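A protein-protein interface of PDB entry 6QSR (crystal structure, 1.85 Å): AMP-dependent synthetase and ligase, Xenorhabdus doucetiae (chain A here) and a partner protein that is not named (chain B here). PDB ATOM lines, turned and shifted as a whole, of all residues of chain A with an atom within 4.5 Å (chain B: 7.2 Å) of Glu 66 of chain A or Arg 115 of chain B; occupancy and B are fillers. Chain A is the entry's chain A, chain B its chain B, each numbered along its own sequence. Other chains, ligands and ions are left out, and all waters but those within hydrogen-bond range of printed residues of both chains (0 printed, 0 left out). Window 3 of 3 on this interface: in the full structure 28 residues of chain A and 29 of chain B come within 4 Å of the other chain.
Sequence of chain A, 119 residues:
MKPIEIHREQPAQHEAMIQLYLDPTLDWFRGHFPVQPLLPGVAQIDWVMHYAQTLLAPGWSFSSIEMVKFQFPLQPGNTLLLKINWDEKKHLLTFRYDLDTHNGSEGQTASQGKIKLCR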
ATOM      1  N   SER A  63     -26.885  -7.896 -12.627  1.00  0.00           N
ATOM      2  CA  SER A  63     -25.441  -7.653 -12.585  1.00  0.00           C
ATOM      3  C   SER A  63     -25.079  -6.194 -12.268  1.00  0.00           C
ATOM      4  O   SER A  63     -24.303  -5.928 -11.347  1.00  0.00           O
ATOM      5  CB  SER A  63     -24.797  -8.061 -13.909  1.00  0.00           C
ATOM      6  OG  SER A  63     -23.396  -7.991 -13.807  1.00  0.00           O
ATOM      7  N   SER A  64     -25.614  -5.255 -13.044  1.00  0.00           N
ATOM      8  CA  SER A  64     -25.310  -3.838 -12.818  1.00  0.00           C
ATOM      9  C   SER A  64     -26.383  -2.915 -13.349  1.00  0.00           C
ATOM     10  O   SER A  64     -27.175  -3.308 -14.203  1.00  0.00           O
ATOM     11  CB  SER A  64     -23.991  -3.465 -13.493  1.00  0.00           C
ATOM     12  OG  SER A  64     -24.101  -3.537 -14.900  1.00  0.00           O
ATOM     13  N   ILE A  65     -26.403  -1.696 -12.810  1.00  0.00           N
ATOM     14  CA  ILE A  65     -27.118  -0.573 -13.406  1.00  0.00           C
ATOM     15  C   ILE A  65     -26.009   0.273 -14.015  1.00  0.00           C
ATOM     16  O   ILE A  65     -25.313   0.996 -13.304  1.00  0.00           O
ATOM     17  CB  ILE A  65     -27.944   0.225 -12.364  1.00  0.00           C
ATOM     18  CG1 ILE A  65     -28.892  -0.708 -11.599  1.00  0.00           C
ATOM     19  CG2 ILE A  65     -28.747   1.335 -13.039  1.00  0.00           C
ATOM     20  CD1 ILE A  65     -29.331  -0.174 -10.250  1.00  0.00           C
ATOM     21  N   GLU A  66     -25.832   0.147 -15.330  1.00  0.00           N
ATOM     22  CA  GLU A  66     -24.858   0.941 -16.063  1.00  0.00           C
ATOM     23  C   GLU A  66     -25.156   2.438 -16.018  1.00  0.00           C
ATOM     24  O   GLU A  66     -24.255   3.248 -15.763  1.00  0.00           O
ATOM     25  CB  GLU A  66     -24.762   0.466 -17.513  1.00  0.00           C
ATOM     26  CG  GLU A  66     -24.151  -0.926 -17.666  1.00  0.00           C
ATOM     27  CD  GLU A  66     -22.745  -1.012 -17.109  1.00  0.00           C
ATOM     28  OE1 GLU A  66     -21.813  -0.497 -17.761  1.00  0.00           O
ATOM     29  OE2 GLU A  66     -22.565  -1.578 -16.008  1.00  0.00           O
ATOM     30  N   MET A  67     -26.416   2.788 -16.246  1.00  0.00           N
ATOM     31  CA  MET A  67     -26.846   4.172 -16.207  1.00  0.00           C
ATOM     32  C   MET A  67     -28.336   4.189 -15.884  1.00  0.00           C
ATOM     33  O   MET A  67     -29.118   3.436 -16.465  1.00  0.00           O
ATOM     34  CB  MET A  67     -26.545   4.849 -17.559  1.00  0.00           C
ATOM     35  CG  MET A  67     -26.920   6.322 -17.657  1.00  0.00           C
ATOM     36  SD  MET A  67     -25.728   7.490 -16.980  1.00  0.00           S
ATOM     37  CE  MET A  67     -24.400   7.407 -18.179  1.00  0.00           C
ATOM     38  N   LYS A 114     -30.232   1.624 -18.190  1.00  0.00           N
ATOM     39  CA  LYS A 114     -29.578   0.467 -18.805  1.00  0.00           C
ATOM     40  C   LYS A 114     -29.034  -0.442 -17.709  1.00  0.00           C
ATOM     41  O   LYS A 114     -28.194  -0.013 -16.903  1.00  0.00           O
ATOM     42  CB  LYS A 114     -28.414   0.921 -19.687  1.00  0.00           C
ATOM     43  CG  LYS A 114     -28.811   1.791 -20.868  1.00  0.00           C
ATOM     44  CD  LYS A 114     -27.620   2.521 -21.463  1.00  0.00           C
ATOM     45  CE  LYS A 114     -26.651   1.574 -22.148  1.00  0.00           C
ATOM     46  NZ  LYS A 114     -25.552   2.334 -22.810  1.00  0.00           N
ATOM     47  N   LYS A 116     -27.354  -4.358 -16.813  1.00  0.00           N
ATOM     48  CA  LYS A 116     -26.753  -5.594 -17.315  1.00  0.00           C
ATOM     49  C   LYS A 116     -27.224  -6.782 -16.486  1.00  0.00           C
ATOM     50  O   LYS A 116     -27.323  -6.701 -15.249  1.00  0.00           O
ATOM     51  CB  LYS A 116     -25.227  -5.518 -17.351  1.00  0.00           C
ATOM     52  CG  LYS A 116     -24.699  -4.439 -18.279  1.00  0.00           C
ATOM     53  CD  LYS A 116     -24.752  -4.832 -19.749  1.00  0.00           C
ATOM     54  CE  LYS A 116     -23.480  -5.512 -20.235  1.00  0.00           C
ATOM     55  NZ  LYS A 116     -23.163  -5.084 -21.625  1.00  0.00           N
ATOM     56  N   ALA B  79     -28.777  -2.053  -3.581  1.00  0.00           N
ATOM     57  CA  ALA B  79     -27.537  -1.313  -3.372  1.00  0.00           C
ATOM     58  C   ALA B  79     -27.659   0.194  -3.633  1.00  0.00           C
ATOM     59  O   ALA B  79     -27.109   1.000  -2.878  1.00  0.00           O
ATOM     60  CB  ALA B  79     -26.419  -1.905  -4.232  1.00  0.00           C
ATOM     61  N   MET B  83     -27.022   2.958  -0.752  1.00  0.00           N
ATOM     62  CA  MET B  83     -26.039   4.021  -1.039  1.00  0.00           C
ATOM     63  C   MET B  83     -26.650   5.421  -1.012  1.00  0.00           C
ATOM     64  O   MET B  83     -26.046   6.361  -0.469  1.00  0.00           O
ATOM     65  CB  MET B  83     -25.341   3.759  -2.371  1.00  0.00           C
ATOM     66  CG  MET B  83     -24.322   2.639  -2.292  1.00  0.00           C
ATOM     67  SD  MET B  83     -23.493   2.348  -3.870  1.00  0.00           S
ATOM     68  CE  MET B  83     -24.585   1.159  -4.608  1.00  0.00           C
ATOM     69  N   GLY B 111     -27.678   7.263 -11.251  1.00  0.00           N
ATOM     70  CA  GLY B 111     -26.621   6.341 -10.872  1.00  0.00           C
ATOM     71  C   GLY B 111     -25.851   5.922 -12.103  1.00  0.00           C
ATOM     72  O   GLY B 111     -26.409   5.884 -13.207  1.00  0.00           O
ATOM     73  N   ARG B 112     -24.573   5.618 -11.907  1.00  0.00           N
ATOM     74  CA  ARG B 112     -23.650   5.312 -12.979  1.00  0.00           C
ATOM     75  C   ARG B 112     -22.774   4.160 -12.544  1.00  0.00           C
ATOM     76  O   ARG B 112     -22.195   4.211 -11.459  1.00  0.00           O
ATOM     77  CB  ARG B 112     -22.757   6.519 -13.277  1.00  0.00           C
ATOM     78  CG  ARG B 112     -23.471   7.647 -13.994  1.00  0.00           C
ATOM     79  CD  ARG B 112     -22.569   8.864 -14.172  1.00  0.00           C
ATOM     80  NE  ARG B 112     -21.691   8.714 -15.337  1.00  0.00           N
ATOM     81  CZ  ARG B 112     -20.495   9.290 -15.494  1.00  0.00           C
ATOM     82  NH1 ARG B 112     -19.964  10.091 -14.562  1.00  0.00           N
ATOM     83  NH2 ARG B 112     -19.810   9.060 -16.612  1.00  0.00           N
ATOM     84  N   ALA B 113     -22.703   3.133 -13.392  1.00  0.00           N
ATOM     85  CA  ALA B 113     -21.883   1.941 -13.173  1.00  0.00           C
ATOM     86  C   ALA B 113     -21.992   1.382 -11.748  1.00  0.00           C
ATOM     87  O   ALA B 113     -20.998   1.135 -11.047  1.00  0.00           O
ATOM     88  CB  ALA B 113     -20.452   2.218 -13.582  1.00  0.00           C
ATOM     89  N   VAL B 114     -23.236   1.198 -11.322  1.00  0.00           N
ATOM     90  CA  VAL B 114     -23.505   0.528 -10.059  1.00  0.00           C
ATOM     91  C   VAL B 114     -23.392  -0.969 -10.348  1.00  0.00           C
ATOM     92  O   VAL B 114     -24.337  -1.593 -10.801  1.00  0.00           O
ATOM     93  CB  VAL B 114     -24.855   0.957  -9.453  1.00  0.00           C
ATOM     94  CG1 VAL B 114     -25.063   0.286  -8.101  1.00  0.00           C
ATOM     95  CG2 VAL B 114     -24.894   2.476  -9.330  1.00  0.00           C
ATOM     96  N   ARG B 115     -22.202  -1.522 -10.108  1.00  0.00           N
ATOM     97  CA  ARG B 115     -21.870  -2.893 -10.497  1.00  0.00           C
ATOM     98  C   ARG B 115     -21.766  -3.780  -9.262  1.00  0.00           C
ATOM     99  O   ARG B 115     -21.055  -3.445  -8.318  1.00  0.00           O
ATOM    100  CB  ARG B 115     -20.559  -2.908 -11.290  1.00  0.00           C
ATOM    101  CG  ARG B 115     -20.634  -2.046 -12.541  1.00  0.00           C
ATOM    102  CD  ARG B 115     -19.632  -2.452 -13.591  1.00  0.00           C
ATOM    103  NE  ARG B 115     -19.852  -1.701 -14.831  1.00  0.00           N
ATOM    104  CZ  ARG B 115     -19.062  -0.749 -15.325  1.00  0.00           C
ATOM    105  NH1 ARG B 115     -17.930  -0.379 -14.716  1.00  0.00           N
ATOM    106  NH2 ARG B 115     -19.402  -0.161 -16.467  1.00  0.00           N
ATOM    107  N   CYS B 116     -22.487  -4.899  -9.296  1.00  0.00           N
ATOM    108  CA  CYS B 116     -22.588  -5.817  -8.166  1.00  0.00           C
ATOM    109  C   CYS B 116     -21.879  -7.125  -8.520  1.00  0.00           C
ATOM    110  O   CYS B 116     -22.066  -7.652  -9.606  1.00  0.00           O
ATOM    111  CB  CYS B 116     -24.069  -6.057  -7.842  1.00  0.00           C
ATOM    112  SG  CYS B 116     -24.420  -6.620  -6.160  1.00  0.00           S
ATOM    113  N   GLN B 117     -21.085  -7.640  -7.584  1.00  0.00           N
ATOM    114  CA  GLN B 117     -20.392  -8.913  -7.768  1.00  0.00           C
ATOM    115  C   GLN B 117     -21.329 -10.110  -7.579  1.00  0.00           C
ATOM    116  O   GLN B 117     -21.000 -11.218  -8.004  1.00  0.00           O
ATOM    117  CB  GLN B 117     -19.233  -9.024  -6.774  1.00  0.00           C
ATOM    118  CG  GLN B 117     -18.167  -7.954  -6.945  1.00  0.00           C
ATOM    119  CD  GLN B 117     -17.466  -8.035  -8.283  1.00  0.00           C
ATOM    120  OE1 GLN B 117     -17.381  -9.102  -8.888  1.00  0.00           O
ATOM    121  NE2 GLN B 117     -16.958  -6.907  -8.752  1.00  0.00           N
ATOM    122  N   VAL B 118     -22.475  -9.886  -6.934  1.00  0.00           N
ATOM    123  CA  VAL B 118     -23.484 -10.929  -6.717  1.00  0.00           C
ATOM    124  C   VAL B 118     -24.872 -10.429  -7.104  1.00  0.00           C
ATOM    125  O   VAL B 118     -25.127  -9.225  -7.054  1.00  0.00           O
ATOM    126  CB  VAL B 118     -23.494 -11.435  -5.253  1.00  0.00           C
ATOM    127  CG1 VAL B 118     -22.178 -12.137  -4.936  1.00  0.00           C
ATOM    128  CG2 VAL B 118     -23.745 -10.318  -4.257  1.00  0.00           C
ATOM    129  N   VAL B 153     -15.282  -6.221  -1.234  1.00  0.00           N
ATOM    130  CA  VAL B 153     -16.088  -5.259  -1.993  1.00  0.00           C
ATOM    131  C   VAL B 153     -17.093  -6.021  -2.864  1.00  0.00           C
ATOM    132  O   VAL B 153     -16.699  -6.844  -3.686  1.00  0.00           O
ATOM    133  CB  VAL B 153     -15.199  -4.357  -2.883  1.00  0.00           C
ATOM    134  CG1 VAL B 153     -16.052  -3.469  -3.770  1.00  0.00           C
ATOM    135  CG2 VAL B 153     -14.256  -3.517  -2.021  1.00  0.00           C
ATOM    136  N   LEU B 154     -18.379  -5.728  -2.676  1.00  0.00           N
ATOM    137  CA  LEU B 154     -19.471  -6.351  -3.426  1.00  0.00           C
ATOM    138  C   LEU B 154     -20.144  -5.437  -4.449  1.00  0.00           C
ATOM    139  O   LEU B 154     -20.712  -5.938  -5.413  1.00  0.00           O
ATOM    140  CB  LEU B 154     -20.538  -6.852  -2.455  1.00  0.00           C
ATOM    141  CG  LEU B 154     -20.110  -7.925  -1.456  1.00  0.00           C
ATOM    142  CD1 LEU B 154     -21.285  -8.245  -0.548  1.00  0.00           C
ATOM    143  CD2 LEU B 154     -19.614  -9.182  -2.149  1.00  0.00           C
ATOM    144  N   VAL B 155     -20.122  -4.121  -4.217  1.00  0.00           N
ATOM    145  CA  VAL B 155     -20.725  -3.143  -5.123  1.00  0.00           C
ATOM    146  C   VAL B 155     -19.843  -1.901  -5.182  1.00  0.00           C
ATOM    147  O   VAL B 155     -19.321  -1.468  -4.156  1.00  0.00           O
ATOM    148  CB  VAL B 155     -22.141  -2.712  -4.653  1.00  0.00           C
ATOM    149  CG1 VAL B 155     -22.816  -1.841  -5.705  1.00  0.00           C
ATOM    150  CG2 VAL B 155     -23.004  -3.921  -4.339  1.00  0.00           C
ATOM    151  N   THR B 156     -19.676  -1.343  -6.378  1.00  0.00           N
ATOM    152  CA  THR B 156     -19.076  -0.016  -6.557  1.00  0.00           C
ATOM    153  C   THR B 156     -20.062   0.797  -7.382  1.00  0.00           C
ATOM    154  O   THR B 156     -20.921   0.224  -8.053  1.00  0.00           O
ATOM    155  CB  THR B 156     -17.694  -0.051  -7.253  1.00  0.00           C
ATOM    156  OG1 THR B 156     -17.790  -0.692  -8.531  1.00  0.00           O
ATOM    157  CG2 THR B 156     -16.667  -0.775  -6.388  1.00  0.00           C
ATOM    158  N   GLY B 157     -19.951   2.121  -7.331  1.00  0.00           N
ATOM    159  CA  GLY B 157     -20.887   2.977  -8.054  1.00  0.00           C
ATOM    160  C   GLY B 157     -20.713   4.462  -7.814  1.00  0.00           C
ATOM    161  O   GLY B 157     -20.007   4.865  -6.880  1.00  0.00           O
ATOM    162  N   ARG B 158     -21.360   5.269  -8.666  1.00  0.00           N
ATOM    163  CA  ARG B 158     -21.523   6.707  -8.433  1.00  0.00           C
ATOM    164  C   ARG B 158     -22.998   7.065  -8.448  1.00  0.00           C
ATOM    165  O   ARG B 158     -23.751   6.579  -9.303  1.00  0.00           O
ATOM    166  CB  ARG B 158     -20.796   7.541  -9.483  1.00  0.00           C
ATOM    167  CG  ARG B 158     -19.287   7.502  -9.357  1.00  0.00           C
ATOM    168  CD  ARG B 158     -18.639   8.568 -10.225  1.00  0.00           C
ATOM    169  NE  ARG B 158     -17.185   8.525 -10.113  1.00  0.00           N
ATOM    170  CZ  ARG B 158     -16.345   9.306 -10.790  1.00  0.00           C
ATOM    171  NH1 ARG B 158     -16.802  10.208 -11.660  1.00  0.00           N
ATOM    172  NH2 ARG B 158     -15.036   9.175 -10.598  1.00  0.00           N
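Ser 63 of chain A touches Arg 115 of chain B. Val 114 of chain B touches Ser 64 of chain A (O to CA, 3.2 Å). Ser 64 of chain A touches Arg 115 of chain B (CB to CA, 3.7 Å). O of Glu 66 of chain A touches CA of Arg 112 of chain B (3.5 Å). Met 67 of chain A touches Gly 111 of chain B (CA to O, 3.5 Å). Arg 112 of chain B touches Met 67 of chain A.
The backbone NH (N) of Arg 115 of chain B lies within hydrogen-bond range of the backbone carbonyl oxygen (O) of Thr 156 of chain B, 3.0 Å away. The side-chain carboxylate (OE2) of Glu 66 of chain A is in hydrogen-bond range of the side-chain hydroxyl (OG) of Ser 64 of chain A (2.7 Å). The side-chain sulfur of Cys 116 of chain B sits at hydrogen-bond distance from the backbone carbonyl oxygen of Val 118 of chain B (2.8 Å). The backbone NH (N) of Glu 66 of chain A is in hydrogen-bond range of the backbone carbonyl oxygen (O) of Lys 114 of chain A (2.8 Å). The backbone NH of Arg 112 of chain B sits at hydrogen-bond distance from the backbone carbonyl oxygen of Arg 158 of chain B (2.9 Å). N of Ser 63 of chain A lies within hydrogen-bond range of O of Lys 116 of chain A (2.9 Å).
The backbone carbonyl oxygen of Ile 65 of chain A lies within hydrogen-bond range of the backbone NH of Ala 113 of chain B, 3.4 Å away. O of Glu 66 of chain A is in hydrogen-bond range of N of Ala 113 of chain B (2.8 Å). The backbone NH (N) of Val 114 of chain B is in hydrogen-bond range of the backbone carbonyl oxygen (O) of Ile 65 of chain A. OE1 of Glu 66 of chain A is in salt-bridge range of NH2 of Arg 115 of chain B (2.8 Å). The backbone NH (N) of Cys 116 of chain B is in hydrogen-bond range of the backbone carbonyl oxygen (O) of Ser 63 of chain A, 2.9 Å away.
Hydrophobic or aromatic side chains of chain A that line the printed part of chain B: Met 67. Printed residues of chain B that touch a printed residue of chain A: Gly 111, Arg 112, Ala 113, Val 114, Arg 115 and Cys 116. Among the printed residues, 11 pairs touch across the chains. Among the printed residues, Asp or Glu carboxylates within 4 Å of a Lys or Arg side-chain nitrogen of the other chain: Glu 66 of chain A with Arg 115 of chain B (2.8 Å).
Of chain B, only Arg 112 (3.5 Å), Ala 113 (2.8 Å) and Arg 115 (2.8 Å) come within 4 Å of Glu 66 of chain A. Of chain A, only Ser 63 (3.9 Å), Ser 64 (3.7 Å) and Glu 66 (2.8 Å) come within 4 Å of Arg 115 of chain B. Printed residues of chain A within 4 Å of Ala 113 of chain B: Ile 65 (3.4 Å) and Glu 66 (2.8 Å). Of the printed residues of chain A, Gly 111 of chain B touches Met 67. Val 155 of chain B touches none of the printed residues of chain A. Leu 154 of chain B touches none of the printed residues of chain A. The nearest printed residue of chain A that does not touch Arg 115 of chain B is Ile 65 of chain A (5.0 Å). The nearest printed residue of chain B that does not touch Ser 63 of chain A is Val 114 of chain B (4.4 Å).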
